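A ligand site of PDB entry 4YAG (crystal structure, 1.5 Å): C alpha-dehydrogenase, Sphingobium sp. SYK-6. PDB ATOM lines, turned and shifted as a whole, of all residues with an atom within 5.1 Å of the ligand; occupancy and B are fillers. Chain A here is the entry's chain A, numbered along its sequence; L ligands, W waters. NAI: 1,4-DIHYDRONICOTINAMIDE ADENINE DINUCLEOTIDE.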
ATOM      1  N   GLY A  12     -15.709 -17.997  27.664  1.00  0.00           N
ATOM      2  CA  GLY A  12     -14.385 -18.337  28.162  1.00  0.00           C
ATOM      3  C   GLY A  12     -14.439 -19.561  29.067  1.00  0.00           C
ATOM      4  O   GLY A  12     -13.599 -19.724  29.954  1.00  0.00           O
ATOM      5  N   ALA A  14     -13.727 -22.617  28.588  1.00  0.00           N
ATOM      6  CA  ALA A  14     -12.805 -23.717  28.313  1.00  0.00           C
ATOM      7  C   ALA A  14     -11.397 -23.517  28.879  1.00  0.00           C
ATOM      8  O   ALA A  14     -10.486 -24.305  28.586  1.00  0.00           O
ATOM      9  CB  ALA A  14     -12.747 -23.969  26.808  1.00  0.00           C
ATOM     10  N   SER A  15     -11.207 -22.476  29.686  1.00  0.00           N
ATOM     11  CA  SER A  15      -9.930 -22.256  30.329  1.00  0.00           C
ATOM     12  C   SER A  15     -10.127 -21.469  31.621  1.00  0.00           C
ATOM     13  O   SER A  15     -11.153 -20.810  31.809  1.00  0.00           O
ATOM     14  CB  SER A  15      -9.017 -21.474  29.396  1.00  0.00           C
ATOM     15  OG  SER A  15      -7.721 -21.302  29.945  1.00  0.00           O
ATOM     16  N   GLY A  16      -9.136 -21.547  32.505  1.00  0.00           N
ATOM     17  CA  GLY A  16      -9.030 -20.580  33.597  1.00  0.00           C
ATOM     18  C   GLY A  16     -10.273 -20.513  34.480  1.00  0.00           C
ATOM     19  O   GLY A  16     -10.838 -21.533  34.870  1.00  0.00           O
ATOM     20  N   ILE A  17     -10.645 -19.297  34.855  1.00  0.00           N
ATOM     21  CA  ILE A  17     -11.778 -19.071  35.741  1.00  0.00           C
ATOM     22  C   ILE A  17     -13.072 -19.688  35.215  1.00  0.00           C
ATOM     23  O   ILE A  17     -13.808 -20.351  35.946  1.00  0.00           O
ATOM     24  CB  ILE A  17     -11.943 -17.568  35.983  1.00  0.00           C
ATOM     25  CG1 ILE A  17     -10.729 -17.034  36.762  1.00  0.00           C
ATOM     26  CG2 ILE A  17     -13.251 -17.258  36.688  1.00  0.00           C
ATOM     27  CD1 ILE A  17     -10.732 -15.517  36.951  1.00  0.00           C
ATOM     28  N   GLY A  18     -13.352 -19.457  33.938  1.00  0.00           N
ATOM     29  CA  GLY A  18     -14.573 -20.002  33.365  1.00  0.00           C
ATOM     30  C   GLY A  18     -14.634 -21.500  33.484  1.00  0.00           C
ATOM     31  O   GLY A  18     -15.679 -22.079  33.734  1.00  0.00           O
ATOM     32  N   ALA A  35     -18.545 -21.629  25.635  1.00  0.00           N
ATOM     33  CA  ALA A  35     -18.372 -20.821  24.442  1.00  0.00           C
ATOM     34  C   ALA A  35     -16.991 -20.159  24.530  1.00  0.00           C
ATOM     35  O   ALA A  35     -16.641 -19.548  25.532  1.00  0.00           O
ATOM     36  CB  ALA A  35     -19.471 -19.758  24.336  1.00  0.00           C
ATOM     37  N   ASP A  36     -16.199 -20.316  23.496  1.00  0.00           N
ATOM     38  CA  ASP A  36     -14.801 -19.874  23.546  1.00  0.00           C
ATOM     39  C   ASP A  36     -14.292 -19.641  22.140  1.00  0.00           C
ATOM     40  O   ASP A  36     -14.691 -20.330  21.190  1.00  0.00           O
ATOM     41  CB  ASP A  36     -13.970 -20.949  24.248  1.00  0.00           C
ATOM     42  CG  ASP A  36     -12.706 -20.428  24.905  1.00  0.00           C
ATOM     43  OD1 ASP A  36     -11.760 -20.066  24.161  1.00  0.00           O
ATOM     44  OD2 ASP A  36     -12.670 -20.383  26.162  1.00  0.00           O
ATOM     45  N   ILE A  37     -13.336 -18.732  22.010  1.00  0.00           N
ATOM     46  CA  ILE A  37     -12.775 -18.420  20.713  1.00  0.00           C
ATOM     47  C   ILE A  37     -11.651 -19.397  20.311  1.00  0.00           C
ATOM     48  O   ILE A  37     -11.261 -19.466  19.152  1.00  0.00           O
ATOM     49  CB  ILE A  37     -12.270 -16.933  20.688  1.00  0.00           C
ATOM     50  CG1 ILE A  37     -12.176 -16.400  19.254  1.00  0.00           C
ATOM     51  CG2 ILE A  37     -10.944 -16.797  21.405  1.00  0.00           C
ATOM     52  CD1 ILE A  37     -11.902 -14.910  19.214  1.00  0.00           C
ATOM     53  N   ARG A  38     -11.154 -20.160  21.285  1.00  0.00           N
ATOM     54  CA  ARG A  38     -10.034 -21.067  21.066  1.00  0.00           C
ATOM     55  C   ARG A  38     -10.500 -22.516  20.908  1.00  0.00           C
ATOM     56  O   ARG A  38     -10.936 -23.133  21.873  1.00  0.00           O
ATOM     57  CB  ARG A  38      -9.042 -20.973  22.230  1.00  0.00           C
ATOM     58  CG  ARG A  38      -8.224 -19.671  22.228  1.00  0.00           C
ATOM     59  CD  ARG A  38      -7.037 -19.726  21.285  1.00  0.00           C
ATOM     60  NE  ARG A  38      -6.073 -20.770  21.653  1.00  0.00           N
ATOM     61  CZ  ARG A  38      -5.121 -20.622  22.568  1.00  0.00           C
ATOM     62  NH1 ARG A  38      -4.999 -19.470  23.233  1.00  0.00           N
ATOM     63  NH2 ARG A  38      -4.324 -21.631  22.856  1.00  0.00           N
ATOM     64  N   HIS A  41      -8.653 -24.952  23.232  1.00  0.00           N
ATOM     65  CA  HIS A  41      -9.181 -24.926  24.594  1.00  0.00           C
ATOM     66  C   HIS A  41     -10.485 -25.738  24.668  1.00  0.00           C
ATOM     67  O   HIS A  41     -10.664 -26.516  25.606  1.00  0.00           O
ATOM     68  CB  HIS A  41      -9.428 -23.487  25.090  1.00  0.00           C
ATOM     69  CG  HIS A  41      -8.181 -22.715  25.314  1.00  0.00           C
ATOM     70  ND1 HIS A  41      -8.193 -21.421  25.838  1.00  0.00           N
ATOM     71  CD2 HIS A  41      -6.871 -22.995  25.139  1.00  0.00           C
ATOM     72  CE1 HIS A  41      -6.975 -20.977  25.966  1.00  0.00           C
ATOM     73  NE2 HIS A  41      -6.133 -21.918  25.528  1.00  0.00           N
ATOM     74  N   LEU A  63     -16.852 -19.351  19.332  1.00  0.00           N
ATOM     75  CA  LEU A  63     -17.365 -18.044  18.947  1.00  0.00           C
ATOM     76  C   LEU A  63     -16.492 -16.957  19.543  1.00  0.00           C
ATOM     77  O   LEU A  63     -15.685 -17.195  20.418  1.00  0.00           O
ATOM     78  CB  LEU A  63     -18.813 -17.847  19.387  1.00  0.00           C
ATOM     79  CG  LEU A  63     -19.178 -17.997  20.854  1.00  0.00           C
ATOM     80  CD1 LEU A  63     -18.683 -16.848  21.719  1.00  0.00           C
ATOM     81  CD2 LEU A  63     -20.695 -18.124  21.012  1.00  0.00           C
ATOM     82  N   ASP A  64     -16.663 -15.758  18.980  1.00  0.00           N
ATOM     83  CA  ASP A  64     -16.092 -14.515  19.489  1.00  0.00           C
ATOM     84  C   ASP A  64     -17.227 -13.722  20.144  1.00  0.00           C
ATOM     85  O   ASP A  64     -18.200 -13.378  19.453  1.00  0.00           O
ATOM     86  CB  ASP A  64     -15.531 -13.747  18.291  1.00  0.00           C
ATOM     87  CG  ASP A  64     -14.973 -12.375  18.636  1.00  0.00           C
ATOM     88  OD1 ASP A  64     -15.006 -11.936  19.803  1.00  0.00           O
ATOM     89  OD2 ASP A  64     -14.475 -11.739  17.679  1.00  0.00           O
ATOM     90  N   VAL A  65     -17.127 -13.435  21.442  1.00  0.00           N
ATOM     91  CA  VAL A  65     -18.201 -12.734  22.179  1.00  0.00           C
ATOM     92  C   VAL A  65     -18.470 -11.338  21.640  1.00  0.00           C
ATOM     93  O   VAL A  65     -19.525 -10.755  21.928  1.00  0.00           O
ATOM     94  CB  VAL A  65     -17.919 -12.651  23.702  1.00  0.00           C
ATOM     95  CG1 VAL A  65     -17.913 -14.047  24.315  1.00  0.00           C
ATOM     96  CG2 VAL A  65     -16.612 -11.910  23.986  1.00  0.00           C
ATOM     97  N   SER A  66     -17.536 -10.796  20.873  1.00  0.00           N
ATOM     98  CA  SER A  66     -17.684  -9.452  20.331  1.00  0.00           C
ATOM     99  C   SER A  66     -18.360  -9.465  18.957  1.00  0.00           C
ATOM    100  O   SER A  66     -18.533  -8.418  18.317  1.00  0.00           O
ATOM    101  CB  SER A  66     -16.352  -8.686  20.313  1.00  0.00           C
ATOM    102  OG  SER A  66     -15.424  -9.248  19.428  1.00  0.00           O
ATOM    103  N   ASN A  91     -17.842 -14.287  31.055  1.00  0.00           N
ATOM    104  CA  ASN A  91     -16.552 -14.379  31.726  1.00  0.00           C
ATOM    105  C   ASN A  91     -15.336 -14.167  30.820  1.00  0.00           C
ATOM    106  O   ASN A  91     -14.272 -13.788  31.307  1.00  0.00           O
ATOM    107  CB  ASN A  91     -16.470 -15.713  32.454  1.00  0.00           C
ATOM    108  CG  ASN A  91     -15.069 -16.132  32.765  1.00  0.00           C
ATOM    109  OD1 ASN A  91     -14.491 -15.749  33.800  1.00  0.00           O
ATOM    110  ND2 ASN A  91     -14.495 -16.931  31.887  1.00  0.00           N
ATOM    111  N   ALA A  92     -15.488 -14.402  29.510  1.00  0.00           N
ATOM    112  CA  ALA A  92     -14.356 -14.243  28.612  1.00  0.00           C
ATOM    113  C   ALA A  92     -13.724 -12.879  28.810  1.00  0.00           C
ATOM    114  O   ALA A  92     -14.406 -11.863  28.979  1.00  0.00           O
ATOM    115  CB  ALA A  92     -14.786 -14.410  27.163  1.00  0.00           C
ATOM    116  N   GLY A  93     -12.409 -12.845  28.696  1.00  0.00           N
ATOM    117  CA  GLY A  93     -11.688 -11.598  28.736  1.00  0.00           C
ATOM    118  C   GLY A  93     -10.278 -11.801  28.304  1.00  0.00           C
ATOM    119  O   GLY A  93      -9.807 -12.932  28.223  1.00  0.00           O
ATOM    120  N   ILE A  94      -9.617 -10.685  28.003  1.00  0.00           N
ATOM    121  CA  ILE A  94      -8.251 -10.703  27.553  1.00  0.00           C
ATOM    122  C   ILE A  94      -7.480  -9.560  28.250  1.00  0.00           C
ATOM    123  O   ILE A  94      -8.062  -8.691  28.893  1.00  0.00           O
ATOM    124  CB  ILE A  94      -8.126 -10.570  26.013  1.00  0.00           C
ATOM    125  CG1 ILE A  94      -9.054  -9.490  25.443  1.00  0.00           C
ATOM    126  CG2 ILE A  94      -8.450 -11.906  25.334  1.00  0.00           C
ATOM    127  CD1 ILE A  94      -8.554  -8.056  25.655  1.00  0.00           C
ATOM    128  N   ILE A 114     -13.898  -6.847  23.771  1.00  0.00           N
ATOM    129  CA  ILE A 114     -13.980  -8.136  24.440  1.00  0.00           C
ATOM    130  C   ILE A 114     -14.456  -7.950  25.878  1.00  0.00           C
ATOM    131  O   ILE A 114     -15.385  -8.602  26.331  1.00  0.00           O
ATOM    132  CB  ILE A 114     -12.644  -8.909  24.418  1.00  0.00           C
ATOM    133  CG1 ILE A 114     -12.039  -8.964  23.010  1.00  0.00           C
ATOM    134  CG2 ILE A 114     -12.839 -10.296  25.020  1.00  0.00           C
ATOM    135  CD1 ILE A 114     -12.991  -9.355  21.909  1.00  0.00           C
ATOM    136  N   ASN A 115     -13.820  -7.031  26.599  1.00  0.00           N
ATOM    137  CA  ASN A 115     -14.015  -6.972  28.045  1.00  0.00           C
ATOM    138  C   ASN A 115     -15.262  -6.196  28.499  1.00  0.00           C
ATOM    139  O   ASN A 115     -15.734  -6.393  29.611  1.00  0.00           O
ATOM    140  CB  ASN A 115     -12.769  -6.413  28.746  1.00  0.00           C
ATOM    141  CG  ASN A 115     -11.575  -7.369  28.696  1.00  0.00           C
ATOM    142  OD1 ASN A 115     -11.706  -8.533  28.330  1.00  0.00           O
ATOM    143  ND2 ASN A 115     -10.403  -6.872  29.046  1.00  0.00           N
ATOM    144  N   THR A 142     -17.681 -11.402  34.813  1.00  0.00           N
ATOM    145  CA  THR A 142     -16.355 -11.356  35.411  1.00  0.00           C
ATOM    146  C   THR A 142     -15.696 -10.028  35.114  1.00  0.00           C
ATOM    147  O   THR A 142     -15.359  -9.731  33.975  1.00  0.00           O
ATOM    148  CB  THR A 142     -15.441 -12.468  34.892  1.00  0.00           C
ATOM    149  OG1 THR A 142     -16.095 -13.734  35.064  1.00  0.00           O
ATOM    150  CG2 THR A 142     -14.136 -12.446  35.669  1.00  0.00           C
ATOM    151  N   ALA A 143     -15.537  -9.214  36.149  1.00  0.00           N
ATOM    152  CA  ALA A 143     -14.800  -7.965  36.013  1.00  0.00           C
ATOM    153  C   ALA A 143     -13.375  -8.228  36.508  1.00  0.00           C
ATOM    154  O   ALA A 143     -12.704  -9.144  36.012  1.00  0.00           O
ATOM    155  CB  ALA A 143     -15.502  -6.851  36.764  1.00  0.00           C
ATOM    156  N   SER A 144     -12.910  -7.458  37.493  1.00  0.00           N
ATOM    157  CA  SER A 144     -11.578  -7.603  38.075  1.00  0.00           C
ATOM    158  C   SER A 144     -11.468  -6.636  39.237  1.00  0.00           C
ATOM    159  O   SER A 144     -12.130  -5.596  39.227  1.00  0.00           O
ATOM    160  CB  SER A 144     -10.502  -7.241  37.060  1.00  0.00           C
ATOM    161  OG  SER A 144      -9.225  -7.285  37.701  1.00  0.00           O
ATOM    162  N   LEU A 145     -10.602  -6.927  40.204  1.00  0.00           N
ATOM    163  CA  LEU A 145     -10.291  -5.927  41.213  1.00  0.00           C
ATOM    164  C   LEU A 145      -9.556  -4.749  40.569  1.00  0.00           C
ATOM    165  O   LEU A 145      -9.544  -3.644  41.114  1.00  0.00           O
ATOM    166  CB  LEU A 145      -9.488  -6.511  42.354  1.00  0.00           C
ATOM    167  CG  LEU A 145     -10.323  -7.382  43.295  1.00  0.00           C
ATOM    168  CD1 LEU A 145      -9.437  -8.166  44.283  1.00  0.00           C
ATOM    169  CD2 LEU A 145     -11.308  -6.536  44.071  1.00  0.00           C
ATOM    170  N   TYR A 158      -7.592  -2.120  30.158  1.00  0.00           N
ATOM    171  CA  TYR A 158      -8.131  -3.187  30.984  1.00  0.00           C
ATOM    172  C   TYR A 158      -8.961  -2.600  32.114  1.00  0.00           C
ATOM    173  O   TYR A 158     -10.115  -2.954  32.308  1.00  0.00           O
ATOM    174  CB  TYR A 158      -7.000  -4.003  31.586  1.00  0.00           C
ATOM    175  CG  TYR A 158      -7.446  -5.278  32.257  1.00  0.00           C
ATOM    176  CD1 TYR A 158      -7.853  -6.373  31.505  1.00  0.00           C
ATOM    177  CD2 TYR A 158      -7.429  -5.409  33.635  1.00  0.00           C
ATOM    178  CE1 TYR A 158      -8.231  -7.567  32.118  1.00  0.00           C
ATOM    179  CE2 TYR A 158      -7.826  -6.605  34.252  1.00  0.00           C
ATOM    180  CZ  TYR A 158      -8.211  -7.667  33.485  1.00  0.00           C
ATOM    181  OH  TYR A 158      -8.587  -8.840  34.118  1.00  0.00           O
ATOM    182  N   LYS A 162     -13.046  -2.918  32.849  1.00  0.00           N
ATOM    183  CA  LYS A 162     -13.461  -3.683  34.008  1.00  0.00           C
ATOM    184  C   LYS A 162     -14.274  -2.850  35.005  1.00  0.00           C
ATOM    185  O   LYS A 162     -15.189  -3.359  35.634  1.00  0.00           O
ATOM    186  CB  LYS A 162     -12.265  -4.337  34.694  1.00  0.00           C
ATOM    187  CG  LYS A 162     -11.581  -5.423  33.834  1.00  0.00           C
ATOM    188  CD  LYS A 162     -12.517  -6.571  33.579  1.00  0.00           C
ATOM    189  CE  LYS A 162     -11.800  -7.804  33.012  1.00  0.00           C
ATOM    190  NZ  LYS A 162     -12.754  -8.905  32.759  1.00  0.00           N
ATOM    191  N   PRO A 188     -11.949 -10.732  40.491  1.00  0.00           N
ATOM    192  CA  PRO A 188     -10.826 -11.508  40.982  1.00  0.00           C
ATOM    193  C   PRO A 188      -9.541 -10.719  41.197  1.00  0.00           C
ATOM    194  O   PRO A 188      -9.280  -9.696  40.542  1.00  0.00           O
ATOM    195  CB  PRO A 188     -10.590 -12.552  39.884  1.00  0.00           C
ATOM    196  CG  PRO A 188     -11.844 -12.566  39.056  1.00  0.00           C
ATOM    197  CD  PRO A 188     -12.335 -11.135  39.122  1.00  0.00           C
ATOM    198  N   GLY A 189      -8.724 -11.260  42.090  1.00  0.00           N
ATOM    199  CA  GLY A 189      -7.299 -11.037  42.151  1.00  0.00           C
ATOM    200  C   GLY A 189      -6.609 -12.111  41.330  1.00  0.00           C
ATOM    201  O   GLY A 189      -7.208 -12.660  40.417  1.00  0.00           O
ATOM    202  N   PRO A 190      -5.361 -12.412  41.638  1.00  0.00           N
ATOM    203  CA  PRO A 190      -4.592 -13.353  40.796  1.00  0.00           C
ATOM    204  C   PRO A 190      -5.063 -14.804  40.864  1.00  0.00           C
ATOM    205  O   PRO A 190      -4.982 -15.440  41.919  1.00  0.00           O
ATOM    206  CB  PRO A 190      -3.169 -13.222  41.331  1.00  0.00           C
ATOM    207  CG  PRO A 190      -3.148 -11.984  42.166  1.00  0.00           C
ATOM    208  CD  PRO A 190      -4.535 -11.798  42.697  1.00  0.00           C
ATOM    209  N   ILE A 191      -5.569 -15.307  39.737  1.00  0.00           N
ATOM    210  CA  ILE A 191      -6.032 -16.685  39.597  1.00  0.00           C
ATOM    211  C   ILE A 191      -5.204 -17.374  38.532  1.00  0.00           C
ATOM    212  O   ILE A 191      -4.912 -16.801  37.486  1.00  0.00           O
ATOM    213  CB  ILE A 191      -7.510 -16.745  39.153  1.00  0.00           C
ATOM    214  CG1 ILE A 191      -8.382 -15.718  39.911  1.00  0.00           C
ATOM    215  CG2 ILE A 191      -8.066 -18.178  39.269  1.00  0.00           C
ATOM    216  CD1 ILE A 191      -8.388 -15.903  41.388  1.00  0.00           C
ATOM    217  N   LYS A 192      -4.829 -18.621  38.800  1.00  0.00           N
ATOM    218  CA  LYS A 192      -4.134 -19.432  37.796  1.00  0.00           C
ATOM    219  C   LYS A 192      -5.007 -19.588  36.559  1.00  0.00           C
ATOM    220  O   LYS A 192      -6.137 -20.039  36.649  1.00  0.00           O
ATOM    221  CB  LYS A 192      -3.795 -20.817  38.332  1.00  0.00           C
ATOM    222  CG  LYS A 192      -2.820 -20.837  39.482  1.00  0.00           C
ATOM    223  CD  LYS A 192      -2.491 -22.274  39.878  1.00  0.00           C
ATOM    224  CE  LYS A 192      -1.590 -22.327  41.095  1.00  0.00           C
ATOM    225  NZ  LYS A 192      -1.478 -23.707  41.636  1.00  0.00           N
ATOM    226  N   SER A 193      -4.466 -19.228  35.407  1.00  0.00           N
ATOM    227  CA  SER A 193      -5.232 -19.276  34.166  1.00  0.00           C
ATOM    228  C   SER A 193      -4.292 -19.208  32.973  1.00  0.00           C
ATOM    229  O   SER A 193      -3.081 -19.261  33.138  1.00  0.00           O
ATOM    230  CB  SER A 193      -6.241 -18.139  34.100  1.00  0.00           C
ATOM    231  OG  SER A 193      -5.605 -16.915  33.710  1.00  0.00           O
ATOM    232  N   ARG A 194      -4.870 -19.065  31.789  1.00  0.00           N
ATOM    233  CA  ARG A 194      -4.076 -18.949  30.573  1.00  0.00           C
ATOM    234  C   ARG A 194      -4.231 -17.586  29.910  1.00  0.00           C
ATOM    235  O   ARG A 194      -4.039 -17.453  28.693  1.00  0.00           O
ATOM    236  CB  ARG A 194      -4.418 -20.084  29.606  1.00  0.00           C
ATOM    237  CG  ARG A 194      -3.906 -21.412  30.124  1.00  0.00           C
ATOM    238  CD  ARG A 194      -4.069 -22.550  29.120  1.00  0.00           C
ATOM    239  NE  ARG A 194      -5.445 -23.029  29.097  1.00  0.00           N
ATOM    240  CZ  ARG A 194      -5.844 -24.103  28.405  1.00  0.00           C
ATOM    241  NH1 ARG A 194      -4.965 -24.753  27.665  1.00  0.00           N
ATOM    242  NH2 ARG A 194      -7.108 -24.494  28.438  1.00  0.00           N
ATOM    243  N   ILE A 195      -4.560 -16.555  30.700  1.00  0.00           N
ATOM    244  CA  ILE A 195      -4.797 -15.225  30.167  1.00  0.00           C
ATOM    245  C   ILE A 195      -3.518 -14.649  29.543  1.00  0.00           C
ATOM    246  O   ILE A 195      -3.574 -13.715  28.739  1.00  0.00           O
ATOM    247  CB  ILE A 195      -5.431 -14.293  31.206  1.00  0.00           C
ATOM    248  CG1 ILE A 195      -5.970 -13.041  30.501  1.00  0.00           C
ATOM    249  CG2 ILE A 195      -4.438 -13.946  32.321  1.00  0.00           C
ATOM    250  CD1 ILE A 195      -7.169 -12.440  31.154  1.00  0.00           C
ATOM    251  N   ASN A 201      -5.447 -14.841  21.395  1.00  0.00           N
ATOM    252  CA  ASN A 201      -6.893 -14.795  21.483  1.00  0.00           C
ATOM    253  C   ASN A 201      -7.480 -13.540  20.849  1.00  0.00           C
ATOM    254  O   ASN A 201      -8.682 -13.465  20.641  1.00  0.00           O
ATOM    255  CB  ASN A 201      -7.353 -14.869  22.946  1.00  0.00           C
ATOM    256  CG  ASN A 201      -6.879 -16.121  23.634  1.00  0.00           C
ATOM    257  OD1 ASN A 201      -6.542 -17.100  22.973  1.00  0.00           O
ATOM    258  ND2 ASN A 201      -6.878 -16.123  24.981  1.00  0.00           N
ATOM    259  N   PRO A 203      -8.998 -11.214  18.380  1.00  0.00           N
ATOM    260  CA  PRO A 203      -9.612 -11.511  17.085  1.00  0.00           C
ATOM    261  C   PRO A 203      -8.836 -10.892  15.918  1.00  0.00           C
ATOM    262  O   PRO A 203      -8.204  -9.852  16.065  1.00  0.00           O
ATOM    263  CB  PRO A 203     -11.008 -10.900  17.196  1.00  0.00           C
ATOM    264  CG  PRO A 203     -11.309 -10.909  18.676  1.00  0.00           C
ATOM    265  CD  PRO A 203      -9.967 -10.628  19.334  1.00  0.00           C
HETATM  266  PA  NAI L   1      -8.109 -17.577  30.348  1.00  0.00           P
HETATM  267  O1A NAI L   1      -7.426 -17.033  29.121  1.00  0.00           O
HETATM  268  O2A NAI L   1      -7.505 -18.819  30.978  1.00  0.00           O
HETATM  269  O5B NAI L   1      -9.626 -17.866  30.041  1.00  0.00           O
HETATM  270  C5B NAI L   1     -10.337 -17.004  29.210  1.00  0.00           C
HETATM  271  C4B NAI L   1     -10.911 -17.781  28.094  1.00  0.00           C
HETATM  272  O4B NAI L   1     -11.731 -16.816  27.363  1.00  0.00           O
HETATM  273  C3B NAI L   1      -9.958 -18.380  27.154  1.00  0.00           C
HETATM  274  O3B NAI L   1     -10.195 -19.783  26.939  1.00  0.00           O
HETATM  275  C2B NAI L   1     -10.096 -17.590  25.943  1.00  0.00           C
HETATM  276  O2B NAI L   1      -9.808 -18.323  24.733  1.00  0.00           O
HETATM  277  C1B NAI L   1     -11.462 -17.066  25.979  1.00  0.00           C
HETATM  278  N9A NAI L   1     -11.656 -15.881  25.196  1.00  0.00           N
HETATM  279  C8A NAI L   1     -10.829 -14.789  25.077  1.00  0.00           C
HETATM  280  N7A NAI L   1     -11.345 -13.907  24.205  1.00  0.00           N
HETATM  281  C5A NAI L   1     -12.542 -14.398  23.738  1.00  0.00           C
HETATM  282  C6A NAI L   1     -13.518 -13.963  22.851  1.00  0.00           C
HETATM  283  N6A NAI L   1     -13.336 -12.780  22.134  1.00  0.00           N
HETATM  284  N1A NAI L   1     -14.621 -14.733  22.628  1.00  0.00           N
HETATM  285  C2A NAI L   1     -14.769 -15.911  23.266  1.00  0.00           C
HETATM  286  N3A NAI L   1     -13.854 -16.376  24.136  1.00  0.00           N
HETATM  287  C4A NAI L   1     -12.739 -15.655  24.378  1.00  0.00           C
HETATM  288  O3  NAI L   1      -8.043 -16.374  31.380  1.00  0.00           O
HETATM  289  PN  NAI L   1      -8.896 -16.084  32.718  1.00  0.00           P
HETATM  290  O1N NAI L   1      -9.628 -17.313  33.240  1.00  0.00           O
HETATM  291  O2N NAI L   1      -7.886 -15.512  33.690  1.00  0.00           O
HETATM  292  O5D NAI L   1      -9.946 -14.963  32.243  1.00  0.00           O
HETATM  293  C5D NAI L   1     -11.317 -15.006  32.624  1.00  0.00           C
HETATM  294  C4D NAI L   1     -11.757 -13.659  33.070  1.00  0.00           C
HETATM  295  O4D NAI L   1     -11.147 -13.382  34.377  1.00  0.00           O
HETATM  296  C3D NAI L   1     -11.359 -12.552  32.190  1.00  0.00           C
HETATM  297  O3D NAI L   1     -12.480 -11.675  31.982  1.00  0.00           O
HETATM  298  C2D NAI L   1     -10.279 -11.858  32.889  1.00  0.00           C
HETATM  299  O2D NAI L   1     -10.214 -10.480  32.507  1.00  0.00           O
HETATM  300  C1D NAI L   1     -10.628 -11.995  34.291  1.00  0.00           C
HETATM  301  N1N NAI L   1      -9.646 -11.862  35.292  1.00  0.00           N
HETATM  302  C2N NAI L   1      -8.620 -12.754  35.479  1.00  0.00           C
HETATM  303  C3N NAI L   1      -7.714 -12.563  36.505  1.00  0.00           C
HETATM  304  C7N NAI L   1      -6.586 -13.520  36.734  1.00  0.00           C
HETATM  305  O7N NAI L   1      -5.678 -13.287  37.554  1.00  0.00           O
HETATM  306  N7N NAI L   1      -6.639 -14.782  36.018  1.00  0.00           N
HETATM  307  C4N NAI L   1      -7.817 -11.487  37.370  1.00  0.00           C
HETATM  308  C5N NAI L   1      -8.887 -10.622  37.203  1.00  0.00           C
HETATM  309  C6N NAI L   1      -9.789 -10.823  36.188  1.00  0.00           C
HETATM  310  O   HOH W   1     -11.885 -18.111  31.915  1.00  0.00           O
HETATM  311  O   HOH W   2      -3.254 -13.867  36.692  1.00  0.00           O
HETATM  312  O   HOH W   3     -10.467 -12.067  22.307  1.00  0.00           O
HETATM  313  O   HOH W   4      -4.566 -10.907  38.542  1.00  0.00           O
HETATM  314  O   HOH W   5      -7.989 -14.893  27.332  1.00  0.00           O
HETATM  315  O   HOH W   6      -6.239 -18.150  27.026  1.00  0.00           O
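OD2 of Asp 36 sits at hydrogen-bond distance from O3B of the ligand (2.7 Å). The side-chain hydroxyl of Ser 193 lies within hydrogen-bond range of an oxygen (O2N) of the ligand, 2.7 Å away. An oxygen (O2A) of the ligand sits at hydrogen-bond distance from the side-chain hydroxyl (OG) of Ser 15 (2.7 Å). The backbone NH (N) of Ile 17 lies within hydrogen-bond range of an oxygen (O1N) of the ligand (2.8 Å). N of Arg 194 is in hydrogen-bond range of O2A of the ligand (2.8 Å). A ring nitrogen (ND1) of His 41 is in hydrogen-bond range of an oxygen (O3B) of the ligand, 2.8 Å away. OH of Tyr 158 sits at hydrogen-bond distance from O2D of the ligand. O of Asn 91 is in hydrogen-bond range of O3D of the ligand, 2.9 Å away. The side-chain amino group of Lys 162 sits at hydrogen-bond distance from an oxygen (O3D) of the ligand (2.9 Å). An oxygen (O7N) of the ligand sits at hydrogen-bond distance from the backbone NH (N) of Ile 191 (3.0 Å). N7N of the ligand sits at hydrogen-bond distance from O of Ile 191. The side-chain carboxylate (OD1) of Asp 64 is in hydrogen-bond range of a nitrogen (N6A) of the ligand, at 3.0 Å. The backbone NH (N) of Val 65 lies within hydrogen-bond range of a nitrogen (N1A) of the ligand. N of Ile 37 is in hydrogen-bond range of N3A of the ligand (3.2 Å). The backbone NH (N) of Ile 195 is in hydrogen-bond range of an oxygen (O1A) of the ligand (3.3 Å). The backbone NH (N) of Gly 93 lies close to an oxygen (O3D) of the ligand.
Water W2 bridges an oxygen (O7N) of the ligand (2.6 Å) and the backbone carbonyl oxygen (O) of Ile 191 (3.5 Å). Water W6 lies within hydrogen-bond range of O1A of the ligand (2.7 Å), O of Arg 194 (2.8 Å) and ND2 of Asn 201 (2.9 Å). Water W3 lies within hydrogen-bond range of a nitrogen (N7A) of the ligand (2.8 Å) and the backbone carbonyl oxygen of Asn 201 (2.8 Å). Water W5 lies within hydrogen-bond range of the backbone carbonyl oxygen of Gly 93 (2.8 Å), an oxygen (O1A) of the ligand (2.8 Å) and the side-chain amide nitrogen of Asn 201 (2.9 Å).
OD1 of Asp 36 sits at hydrogen-bond distance from N of Arg 38, at 2.9 Å. The side-chain carboxylate of Asp 36 is in hydrogen-bond range of the backbone NH of Ala 14, 3.5 Å away. A ring nitrogen (NE2) of His 41 sits at hydrogen-bond distance from the guanidinium group of Arg 38, at 3.2 Å. The side-chain hydroxyl of Thr 142 is in hydrogen-bond range of the side-chain amide oxygen of Asn 91, at 2.9 Å. The backbone NH of Gly 18 lies close to the side-chain amide nitrogen of Asn 91. The backbone carbonyl oxygen of Thr 142 lies within hydrogen-bond range of the side-chain amino group of Lys 162. OG of Ser 66 sits at hydrogen-bond distance from OD1 of Asp 64, 2.7 Å away. The backbone NH (N) of Ile 37 sits close to the backbone carbonyl oxygen (O) of Leu 63, at 3.2 Å.
O of Leu 63 lies close to N1A of the ligand. The backbone carbonyl oxygen (O) of Gly 189 lies close to an oxygen (O7N) of the ligand, 3.3 Å away. CA of Gly 12 touches O4B of the ligand (3.2 Å). Gly 16 touches the ligand. Arg 38 touches the ligand. Ala 92 touches the ligand (O to O3D, 3.6 Å). Ile 94 touches the ligand (CG2 to N7A, 3.7 Å). Ile 114 touches the ligand (CD1 to N6A, 3.4 Å). Thr 142 touches the ligand (CG2 to O4D, 3.4 Å). Ala 143 touches the ligand. OG of Ser 144 touches C5N of the ligand, at 3.4 Å. Pro 188 touches the ligand. CA of Pro 190 touches O7N of the ligand, at 3.4 Å. ND2 of Asn 201 touches C2B of the ligand, at 3.7 Å. Hydrophobic or aromatic side chains that line the ligand: Ile 17, Ile 37, His 41, Val 65, Ala 92, Ile 94, Ile 114, Tyr 158, Pro 188, Ile 191 and Ile 195.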
